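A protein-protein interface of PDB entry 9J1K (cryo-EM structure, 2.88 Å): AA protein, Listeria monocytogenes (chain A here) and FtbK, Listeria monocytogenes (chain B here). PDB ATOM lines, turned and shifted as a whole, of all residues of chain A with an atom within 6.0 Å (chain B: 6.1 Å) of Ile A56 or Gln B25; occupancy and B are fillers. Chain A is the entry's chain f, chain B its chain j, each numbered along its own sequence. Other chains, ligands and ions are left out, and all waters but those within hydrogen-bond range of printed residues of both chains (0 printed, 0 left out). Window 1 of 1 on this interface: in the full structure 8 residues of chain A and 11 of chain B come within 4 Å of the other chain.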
ATOM      1  N   ILE A  54     -20.495 -29.918 -15.581  1.00  0.00           N
ATOM      2  CA  ILE A  54     -20.978 -28.603 -15.985  1.00  0.00           C
ATOM      3  C   ILE A  54     -21.906 -28.789 -17.174  1.00  0.00           C
ATOM      4  O   ILE A  54     -21.517 -29.388 -18.184  1.00  0.00           O
ATOM      5  CB  ILE A  54     -19.816 -27.657 -16.330  1.00  0.00           C
ATOM      6  CG1 ILE A  54     -18.799 -27.634 -15.189  1.00  0.00           C
ATOM      7  CG2 ILE A  54     -20.337 -26.260 -16.611  1.00  0.00           C
ATOM      8  CD1 ILE A  54     -17.387 -27.359 -15.638  1.00  0.00           C
ATOM      9  N   GLU A  55     -23.126 -28.275 -17.056  1.00  0.00           N
ATOM     10  CA  GLU A  55     -24.150 -28.465 -18.075  1.00  0.00           C
ATOM     11  C   GLU A  55     -24.028 -27.372 -19.129  1.00  0.00           C
ATOM     12  O   GLU A  55     -24.139 -26.182 -18.816  1.00  0.00           O
ATOM     13  CB  GLU A  55     -25.542 -28.454 -17.447  1.00  0.00           C
ATOM     14  CG  GLU A  55     -26.582 -29.215 -18.248  1.00  0.00           C
ATOM     15  CD  GLU A  55     -27.958 -29.161 -17.617  1.00  0.00           C
ATOM     16  OE1 GLU A  55     -28.040 -29.061 -16.375  1.00  0.00           O
ATOM     17  OE2 GLU A  55     -28.958 -29.220 -18.363  1.00  0.00           O
ATOM     18  N   ILE A  56     -23.802 -27.780 -20.375  1.00  0.00           N
ATOM     19  CA  ILE A  56     -23.669 -26.853 -21.492  1.00  0.00           C
ATOM     20  C   ILE A  56     -24.712 -27.192 -22.546  1.00  0.00           C
ATOM     21  O   ILE A  56     -24.462 -27.058 -23.748  1.00  0.00           O
ATOM     22  CB  ILE A  56     -22.250 -26.888 -22.084  1.00  0.00           C
ATOM     23  CG1 ILE A  56     -21.845 -28.326 -22.412  1.00  0.00           C
ATOM     24  CG2 ILE A  56     -21.260 -26.260 -21.122  1.00  0.00           C
ATOM     25  CD1 ILE A  56     -20.796 -28.428 -23.494  1.00  0.00           C
ATOM     26  N   THR A  57     -25.882 -27.648 -22.097  1.00  0.00           N
ATOM     27  CA  THR A  57     -26.939 -28.071 -23.007  1.00  0.00           C
ATOM     28  C   THR A  57     -27.292 -26.962 -23.989  1.00  0.00           C
ATOM     29  O   THR A  57     -27.511 -25.813 -23.598  1.00  0.00           O
ATOM     30  CB  THR A  57     -28.181 -28.477 -22.212  1.00  0.00           C
ATOM     31  OG1 THR A  57     -27.826 -29.466 -21.240  1.00  0.00           O
ATOM     32  CG2 THR A  57     -29.242 -29.042 -23.137  1.00  0.00           C
ATOM     33  N   SER A  58     -27.344 -27.318 -25.267  1.00  0.00           N
ATOM     34  CA  SER A  58     -27.648 -26.382 -26.345  1.00  0.00           C
ATOM     35  C   SER A  58     -28.992 -26.783 -26.944  1.00  0.00           C
ATOM     36  O   SER A  58     -29.097 -27.801 -27.633  1.00  0.00           O
ATOM     37  CB  SER A  58     -26.543 -26.385 -27.394  1.00  0.00           C
ATOM     38  OG  SER A  58     -26.978 -27.018 -28.581  1.00  0.00           O
ATOM     39  N   LYS A  59     -30.019 -25.974 -26.681  1.00  0.00           N
ATOM     40  CA  LYS A  59     -31.363 -26.281 -27.151  1.00  0.00           C
ATOM     41  C   LYS A  59     -31.557 -25.989 -28.631  1.00  0.00           C
ATOM     42  O   LYS A  59     -32.612 -26.328 -29.175  1.00  0.00           O
ATOM     43  CB  LYS A  59     -32.390 -25.497 -26.334  1.00  0.00           C
ATOM     44  CG  LYS A  59     -32.883 -26.229 -25.100  1.00  0.00           C
ATOM     45  CD  LYS A  59     -33.229 -25.258 -23.988  1.00  0.00           C
ATOM     46  CE  LYS A  59     -33.149 -25.928 -22.629  1.00  0.00           C
ATOM     47  NZ  LYS A  59     -34.030 -25.262 -21.633  1.00  0.00           N
ATOM     48  N   ASP A  60     -30.581 -25.372 -29.292  1.00  0.00           N
ATOM     49  CA  ASP A  60     -30.692 -25.017 -30.699  1.00  0.00           C
ATOM     50  C   ASP A  60     -30.016 -26.025 -31.618  1.00  0.00           C
ATOM     51  O   ASP A  60     -29.892 -25.767 -32.819  1.00  0.00           O
ATOM     52  CB  ASP A  60     -30.113 -23.623 -30.937  1.00  0.00           C
ATOM     53  CG  ASP A  60     -31.148 -22.530 -30.774  1.00  0.00           C
ATOM     54  OD1 ASP A  60     -32.252 -22.826 -30.272  1.00  0.00           O
ATOM     55  OD2 ASP A  60     -30.857 -21.374 -31.147  1.00  0.00           O
ATOM     56  N   THR A  61     -29.578 -27.161 -31.086  1.00  0.00           N
ATOM     57  CA  THR A  61     -28.946 -28.209 -31.873  1.00  0.00           C
ATOM     58  C   THR A  61     -29.869 -29.418 -31.945  1.00  0.00           C
ATOM     59  O   THR A  61     -30.602 -29.707 -30.996  1.00  0.00           O
ATOM     60  CB  THR A  61     -27.598 -28.617 -31.273  1.00  0.00           C
ATOM     61  OG1 THR A  61     -26.915 -27.450 -30.799  1.00  0.00           O
ATOM     62  CG2 THR A  61     -26.736 -29.310 -32.315  1.00  0.00           C
ATOM     63  N   SER A  67     -26.132 -31.795 -22.659  1.00  0.00           N
ATOM     64  CA  SER A  67     -24.694 -31.877 -22.857  1.00  0.00           C
ATOM     65  C   SER A  67     -23.968 -31.442 -21.592  1.00  0.00           C
ATOM     66  O   SER A  67     -24.300 -30.414 -20.996  1.00  0.00           O
ATOM     67  CB  SER A  67     -24.251 -31.010 -24.038  1.00  0.00           C
ATOM     68  OG  SER A  67     -25.148 -31.140 -25.126  1.00  0.00           O
ATOM     69  N   LYS A  68     -22.978 -32.234 -21.189  1.00  0.00           N
ATOM     70  CA  LYS A  68     -22.204 -31.970 -19.988  1.00  0.00           C
ATOM     71  C   LYS A  68     -20.720 -32.103 -20.296  1.00  0.00           C
ATOM     72  O   LYS A  68     -20.314 -32.807 -21.224  1.00  0.00           O
ATOM     73  CB  LYS A  68     -22.580 -32.925 -18.845  1.00  0.00           C
ATOM     74  CG  LYS A  68     -24.059 -33.250 -18.750  1.00  0.00           C
ATOM     75  CD  LYS A  68     -24.481 -33.462 -17.307  1.00  0.00           C
ATOM     76  CE  LYS A  68     -25.944 -33.855 -17.214  1.00  0.00           C
ATOM     77  NZ  LYS A  68     -26.224 -35.107 -17.964  1.00  0.00           N
ATOM     78  N   ILE A  69     -19.910 -31.409 -19.498  1.00  0.00           N
ATOM     79  CA  ILE A  69     -18.460 -31.502 -19.577  1.00  0.00           C
ATOM     80  C   ILE A  69     -17.911 -31.700 -18.173  1.00  0.00           C
ATOM     81  O   ILE A  69     -18.575 -31.419 -17.172  1.00  0.00           O
ATOM     82  CB  ILE A  69     -17.815 -30.264 -20.233  1.00  0.00           C
ATOM     83  CG1 ILE A  69     -18.590 -29.000 -19.868  1.00  0.00           C
ATOM     84  CG2 ILE A  69     -17.752 -30.435 -21.741  1.00  0.00           C
ATOM     85  CD1 ILE A  69     -17.961 -27.734 -20.404  1.00  0.00           C
ATOM     86  N   SER B   2     -25.905 -24.100 -33.648  1.00  0.00           N
ATOM     87  CA  SER B   2     -26.250 -22.688 -33.569  1.00  0.00           C
ATOM     88  C   SER B   2     -24.990 -21.840 -33.666  1.00  0.00           C
ATOM     89  O   SER B   2     -23.939 -22.210 -33.136  1.00  0.00           O
ATOM     90  CB  SER B   2     -26.987 -22.375 -32.267  1.00  0.00           C
ATOM     91  OG  SER B   2     -26.461 -23.129 -31.190  1.00  0.00           O
ATOM     92  N   SER B  23     -18.518 -21.603 -28.194  1.00  0.00           N
ATOM     93  CA  SER B  23     -19.613 -22.146 -28.983  1.00  0.00           C
ATOM     94  C   SER B  23     -20.932 -21.596 -28.464  1.00  0.00           C
ATOM     95  O   SER B  23     -21.143 -21.515 -27.251  1.00  0.00           O
ATOM     96  CB  SER B  23     -19.629 -23.677 -28.933  1.00  0.00           C
ATOM     97  OG  SER B  23     -20.086 -24.139 -27.676  1.00  0.00           O
ATOM     98  N   VAL B  24     -21.818 -21.233 -29.386  1.00  0.00           N
ATOM     99  CA  VAL B  24     -23.099 -20.628 -29.033  1.00  0.00           C
ATOM    100  C   VAL B  24     -24.088 -21.746 -28.720  1.00  0.00           C
ATOM    101  O   VAL B  24     -24.467 -22.518 -29.603  1.00  0.00           O
ATOM    102  CB  VAL B  24     -23.622 -19.727 -30.156  1.00  0.00           C
ATOM    103  CG1 VAL B  24     -25.027 -19.247 -29.836  1.00  0.00           C
ATOM    104  CG2 VAL B  24     -22.686 -18.550 -30.369  1.00  0.00           C
ATOM    105  N   GLN B  25     -24.506 -21.836 -27.457  1.00  0.00           N
ATOM    106  CA  GLN B  25     -25.463 -22.867 -27.069  1.00  0.00           C
ATOM    107  C   GLN B  25     -26.854 -22.563 -27.610  1.00  0.00           C
ATOM    108  O   GLN B  25     -27.516 -23.440 -28.177  1.00  0.00           O
ATOM    109  CB  GLN B  25     -25.507 -23.002 -25.548  1.00  0.00           C
ATOM    110  CG  GLN B  25     -24.443 -23.901 -24.964  1.00  0.00           C
ATOM    111  CD  GLN B  25     -24.242 -23.660 -23.485  1.00  0.00           C
ATOM    112  OE1 GLN B  25     -23.114 -23.514 -23.016  1.00  0.00           O
ATOM    113  NE2 GLN B  25     -25.338 -23.612 -22.739  1.00  0.00           N
ATOM    114  N   GLU B  26     -27.314 -21.325 -27.447  1.00  0.00           N
ATOM    115  CA  GLU B  26     -28.703 -21.014 -27.757  1.00  0.00           C
ATOM    116  C   GLU B  26     -28.846 -19.515 -27.972  1.00  0.00           C
ATOM    117  O   GLU B  26     -28.053 -18.727 -27.456  1.00  0.00           O
ATOM    118  CB  GLU B  26     -29.625 -21.501 -26.629  1.00  0.00           C
ATOM    119  CG  GLU B  26     -31.094 -21.147 -26.775  1.00  0.00           C
ATOM    120  CD  GLU B  26     -31.846 -21.242 -25.463  1.00  0.00           C
ATOM    121  OE1 GLU B  26     -31.417 -22.022 -24.588  1.00  0.00           O
ATOM    122  OE2 GLU B  26     -32.864 -20.534 -25.306  1.00  0.00           O
ATOM    123  N   VAL B  27     -29.858 -19.129 -28.746  1.00  0.00           N
ATOM    124  CA  VAL B  27     -30.191 -17.728 -28.953  1.00  0.00           C
ATOM    125  C   VAL B  27     -31.643 -17.508 -28.550  1.00  0.00           C
ATOM    126  O   VAL B  27     -32.463 -18.430 -28.549  1.00  0.00           O
ATOM    127  CB  VAL B  27     -29.954 -17.271 -30.408  1.00  0.00           C
ATOM    128  CG1 VAL B  27     -28.571 -17.687 -30.878  1.00  0.00           C
ATOM    129  CG2 VAL B  27     -31.025 -17.833 -31.325  1.00  0.00           C
ATOM    130  N   LYS B  62     -26.807 -17.451 -25.220  1.00  0.00           N
ATOM    131  CA  LYS B  62     -26.147 -18.260 -24.206  1.00  0.00           C
ATOM    132  C   LYS B  62     -25.067 -19.100 -24.874  1.00  0.00           C
ATOM    133  O   LYS B  62     -25.354 -19.847 -25.819  1.00  0.00           O
ATOM    134  CB  LYS B  62     -27.160 -19.152 -23.489  1.00  0.00           C
ATOM    135  CG  LYS B  62     -26.602 -19.894 -22.292  1.00  0.00           C
ATOM    136  CD  LYS B  62     -27.669 -20.094 -21.232  1.00  0.00           C
ATOM    137  CE  LYS B  62     -28.583 -21.253 -21.586  1.00  0.00           C
ATOM    138  NZ  LYS B  62     -28.914 -22.080 -20.395  1.00  0.00           N
ATOM    139  N   CYS B  63     -23.830 -18.969 -24.391  1.00  0.00           N
ATOM    140  CA  CYS B  63     -22.680 -19.653 -24.962  1.00  0.00           C
ATOM    141  C   CYS B  63     -21.757 -20.110 -23.840  1.00  0.00           C
ATOM    142  O   CYS B  63     -21.947 -19.777 -22.666  1.00  0.00           O
ATOM    143  CB  CYS B  63     -21.915 -18.750 -25.937  1.00  0.00           C
ATOM    144  SG  CYS B  63     -22.765 -17.224 -26.395  1.00  0.00           S
ATOM    145  N   ASN B  64     -20.740 -20.882 -24.215  1.00  0.00           N
ATOM    146  CA  ASN B  64     -19.727 -21.337 -23.276  1.00  0.00           C
ATOM    147  C   ASN B  64     -18.365 -21.289 -23.949  1.00  0.00           C
ATOM    148  O   ASN B  64     -18.251 -21.444 -25.168  1.00  0.00           O
ATOM    149  CB  ASN B  64     -20.010 -22.758 -22.778  1.00  0.00           C
ATOM    150  CG  ASN B  64     -19.988 -23.780 -23.893  1.00  0.00           C
ATOM    151  OD1 ASN B  64     -18.934 -24.310 -24.244  1.00  0.00           O
ATOM    152  ND2 ASN B  64     -21.152 -24.061 -24.460  1.00  0.00           N
ATOM    153  N   GLN B  66     -14.543 -23.004 -23.799  1.00  0.00           N
ATOM    154  CA  GLN B  66     -13.734 -24.131 -23.349  1.00  0.00           C
ATOM    155  C   GLN B  66     -12.315 -23.922 -23.863  1.00  0.00           C
ATOM    156  O   GLN B  66     -12.078 -23.961 -25.074  1.00  0.00           O
ATOM    157  CB  GLN B  66     -14.309 -25.455 -23.847  1.00  0.00           C
ATOM    158  CG  GLN B  66     -15.480 -25.969 -23.034  1.00  0.00           C
ATOM    159  CD  GLN B  66     -16.354 -26.925 -23.817  1.00  0.00           C
ATOM    160  OE1 GLN B  66     -16.016 -28.097 -23.985  1.00  0.00           O
ATOM    161  NE2 GLN B  66     -17.485 -26.431 -24.304  1.00  0.00           N
ATOM    162  N   VAL B 118     -13.151 -23.805 -18.267  1.00  0.00           N
ATOM    163  CA  VAL B 118     -14.445 -23.576 -18.894  1.00  0.00           C
ATOM    164  C   VAL B 118     -15.125 -22.391 -18.221  1.00  0.00           C
ATOM    165  O   VAL B 118     -14.919 -22.116 -17.034  1.00  0.00           O
ATOM    166  CB  VAL B 118     -15.340 -24.837 -18.843  1.00  0.00           C
ATOM    167  CG1 VAL B 118     -14.528 -26.049 -18.419  1.00  0.00           C
ATOM    168  CG2 VAL B 118     -16.530 -24.637 -17.914  1.00  0.00           C
ATOM    169  N   LEU B 120     -19.080 -20.206 -18.533  1.00  0.00           N
ATOM    170  CA  LEU B 120     -20.360 -19.920 -19.161  1.00  0.00           C
ATOM    171  C   LEU B 120     -20.501 -18.426 -19.417  1.00  0.00           C
ATOM    172  O   LEU B 120     -19.846 -17.600 -18.774  1.00  0.00           O
ATOM    173  CB  LEU B 120     -21.510 -20.412 -18.284  1.00  0.00           C
ATOM    174  CG  LEU B 120     -21.404 -21.858 -17.802  1.00  0.00           C
ATOM    175  CD1 LEU B 120     -22.628 -22.243 -16.991  1.00  0.00           C
ATOM    176  CD2 LEU B 120     -21.219 -22.801 -18.979  1.00  0.00           C
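O of Thr A57 lies within hydrogen-bond range of NE2 of Gln B25 (3.2 Å).
The side-chain carboxylate (OD2) of Asp A60 is in hydrogen-bond range of the backbone NH (N) of Val B27, 3.4 Å away.
N of Ile A69 lies within hydrogen-bond range of O of Ile A54, 2.9 Å away.
The backbone NH of Ile A56 lies within hydrogen-bond range of the backbone carbonyl oxygen of Ser A67, 2.8 Å away.
The side-chain hydroxyl (OG1) of Thr A57 is in hydrogen-bond range of the backbone NH (N) of Ser A67 (3.2 Å).
The backbone carbonyl oxygen (O) of Val B24 sits at hydrogen-bond distance from the side-chain hydroxyl (OG) of Ser B2, 2.6 Å away.
The backbone NH (N) of Gln B25 sits at hydrogen-bond distance from the backbone carbonyl oxygen (O) of Lys B62 (2.7 Å).
OE1 of Gln B25 lies within hydrogen-bond range of ND2 of Asn B64.
Among the printed residues, pairs that only touch across the chains: Ser A58 with Gln B25, Ile A56 with Gln B25, Asp A60 with Ser B2, Ile A54 with Val B118, Ile A69 with Gln B66, Lys A59 with Glu B26, Asp A60 with Gln B25, Ile A56 with Asn B64, Lys A59 with Gln B25 and Ile A56 with Gln B66.
Of chain B, only Gln B25 (3.4 Å), Asn B64 (3.9 Å) and Gln B66 (3.95 Å) come within 4 Å of Ile A56.
Gln B25 touches five residues of chain A.
Printed residues of chain B within 4 Å of Thr A57: Gln B25.
Of the printed residues of chain A, Gln B66 touches Ile A56 and Ile A69.
Printed residues of chain B within 4 Å of Ile A69: Gln B66.
Of the printed residues of chain A, Glu B26 touches Lys A59 (3.8 Å).
The nearest residue of chain B that does not touch Ile A56 is Leu B120 (4.1 Å).
Of the 11 printed residues of chain A, 7 touch a printed residue of chain B.
Hydrophobic or aromatic side chains of chain A that line the printed part of chain B: Ile A54, Ile A56 and Ile A69.
Of the 12 printed residues of chain B, 7 touch a printed residue of chain A.
Hydrophobic or aromatic side chains of chain B that line the printed part of chain A: Val B27 and Val B118.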
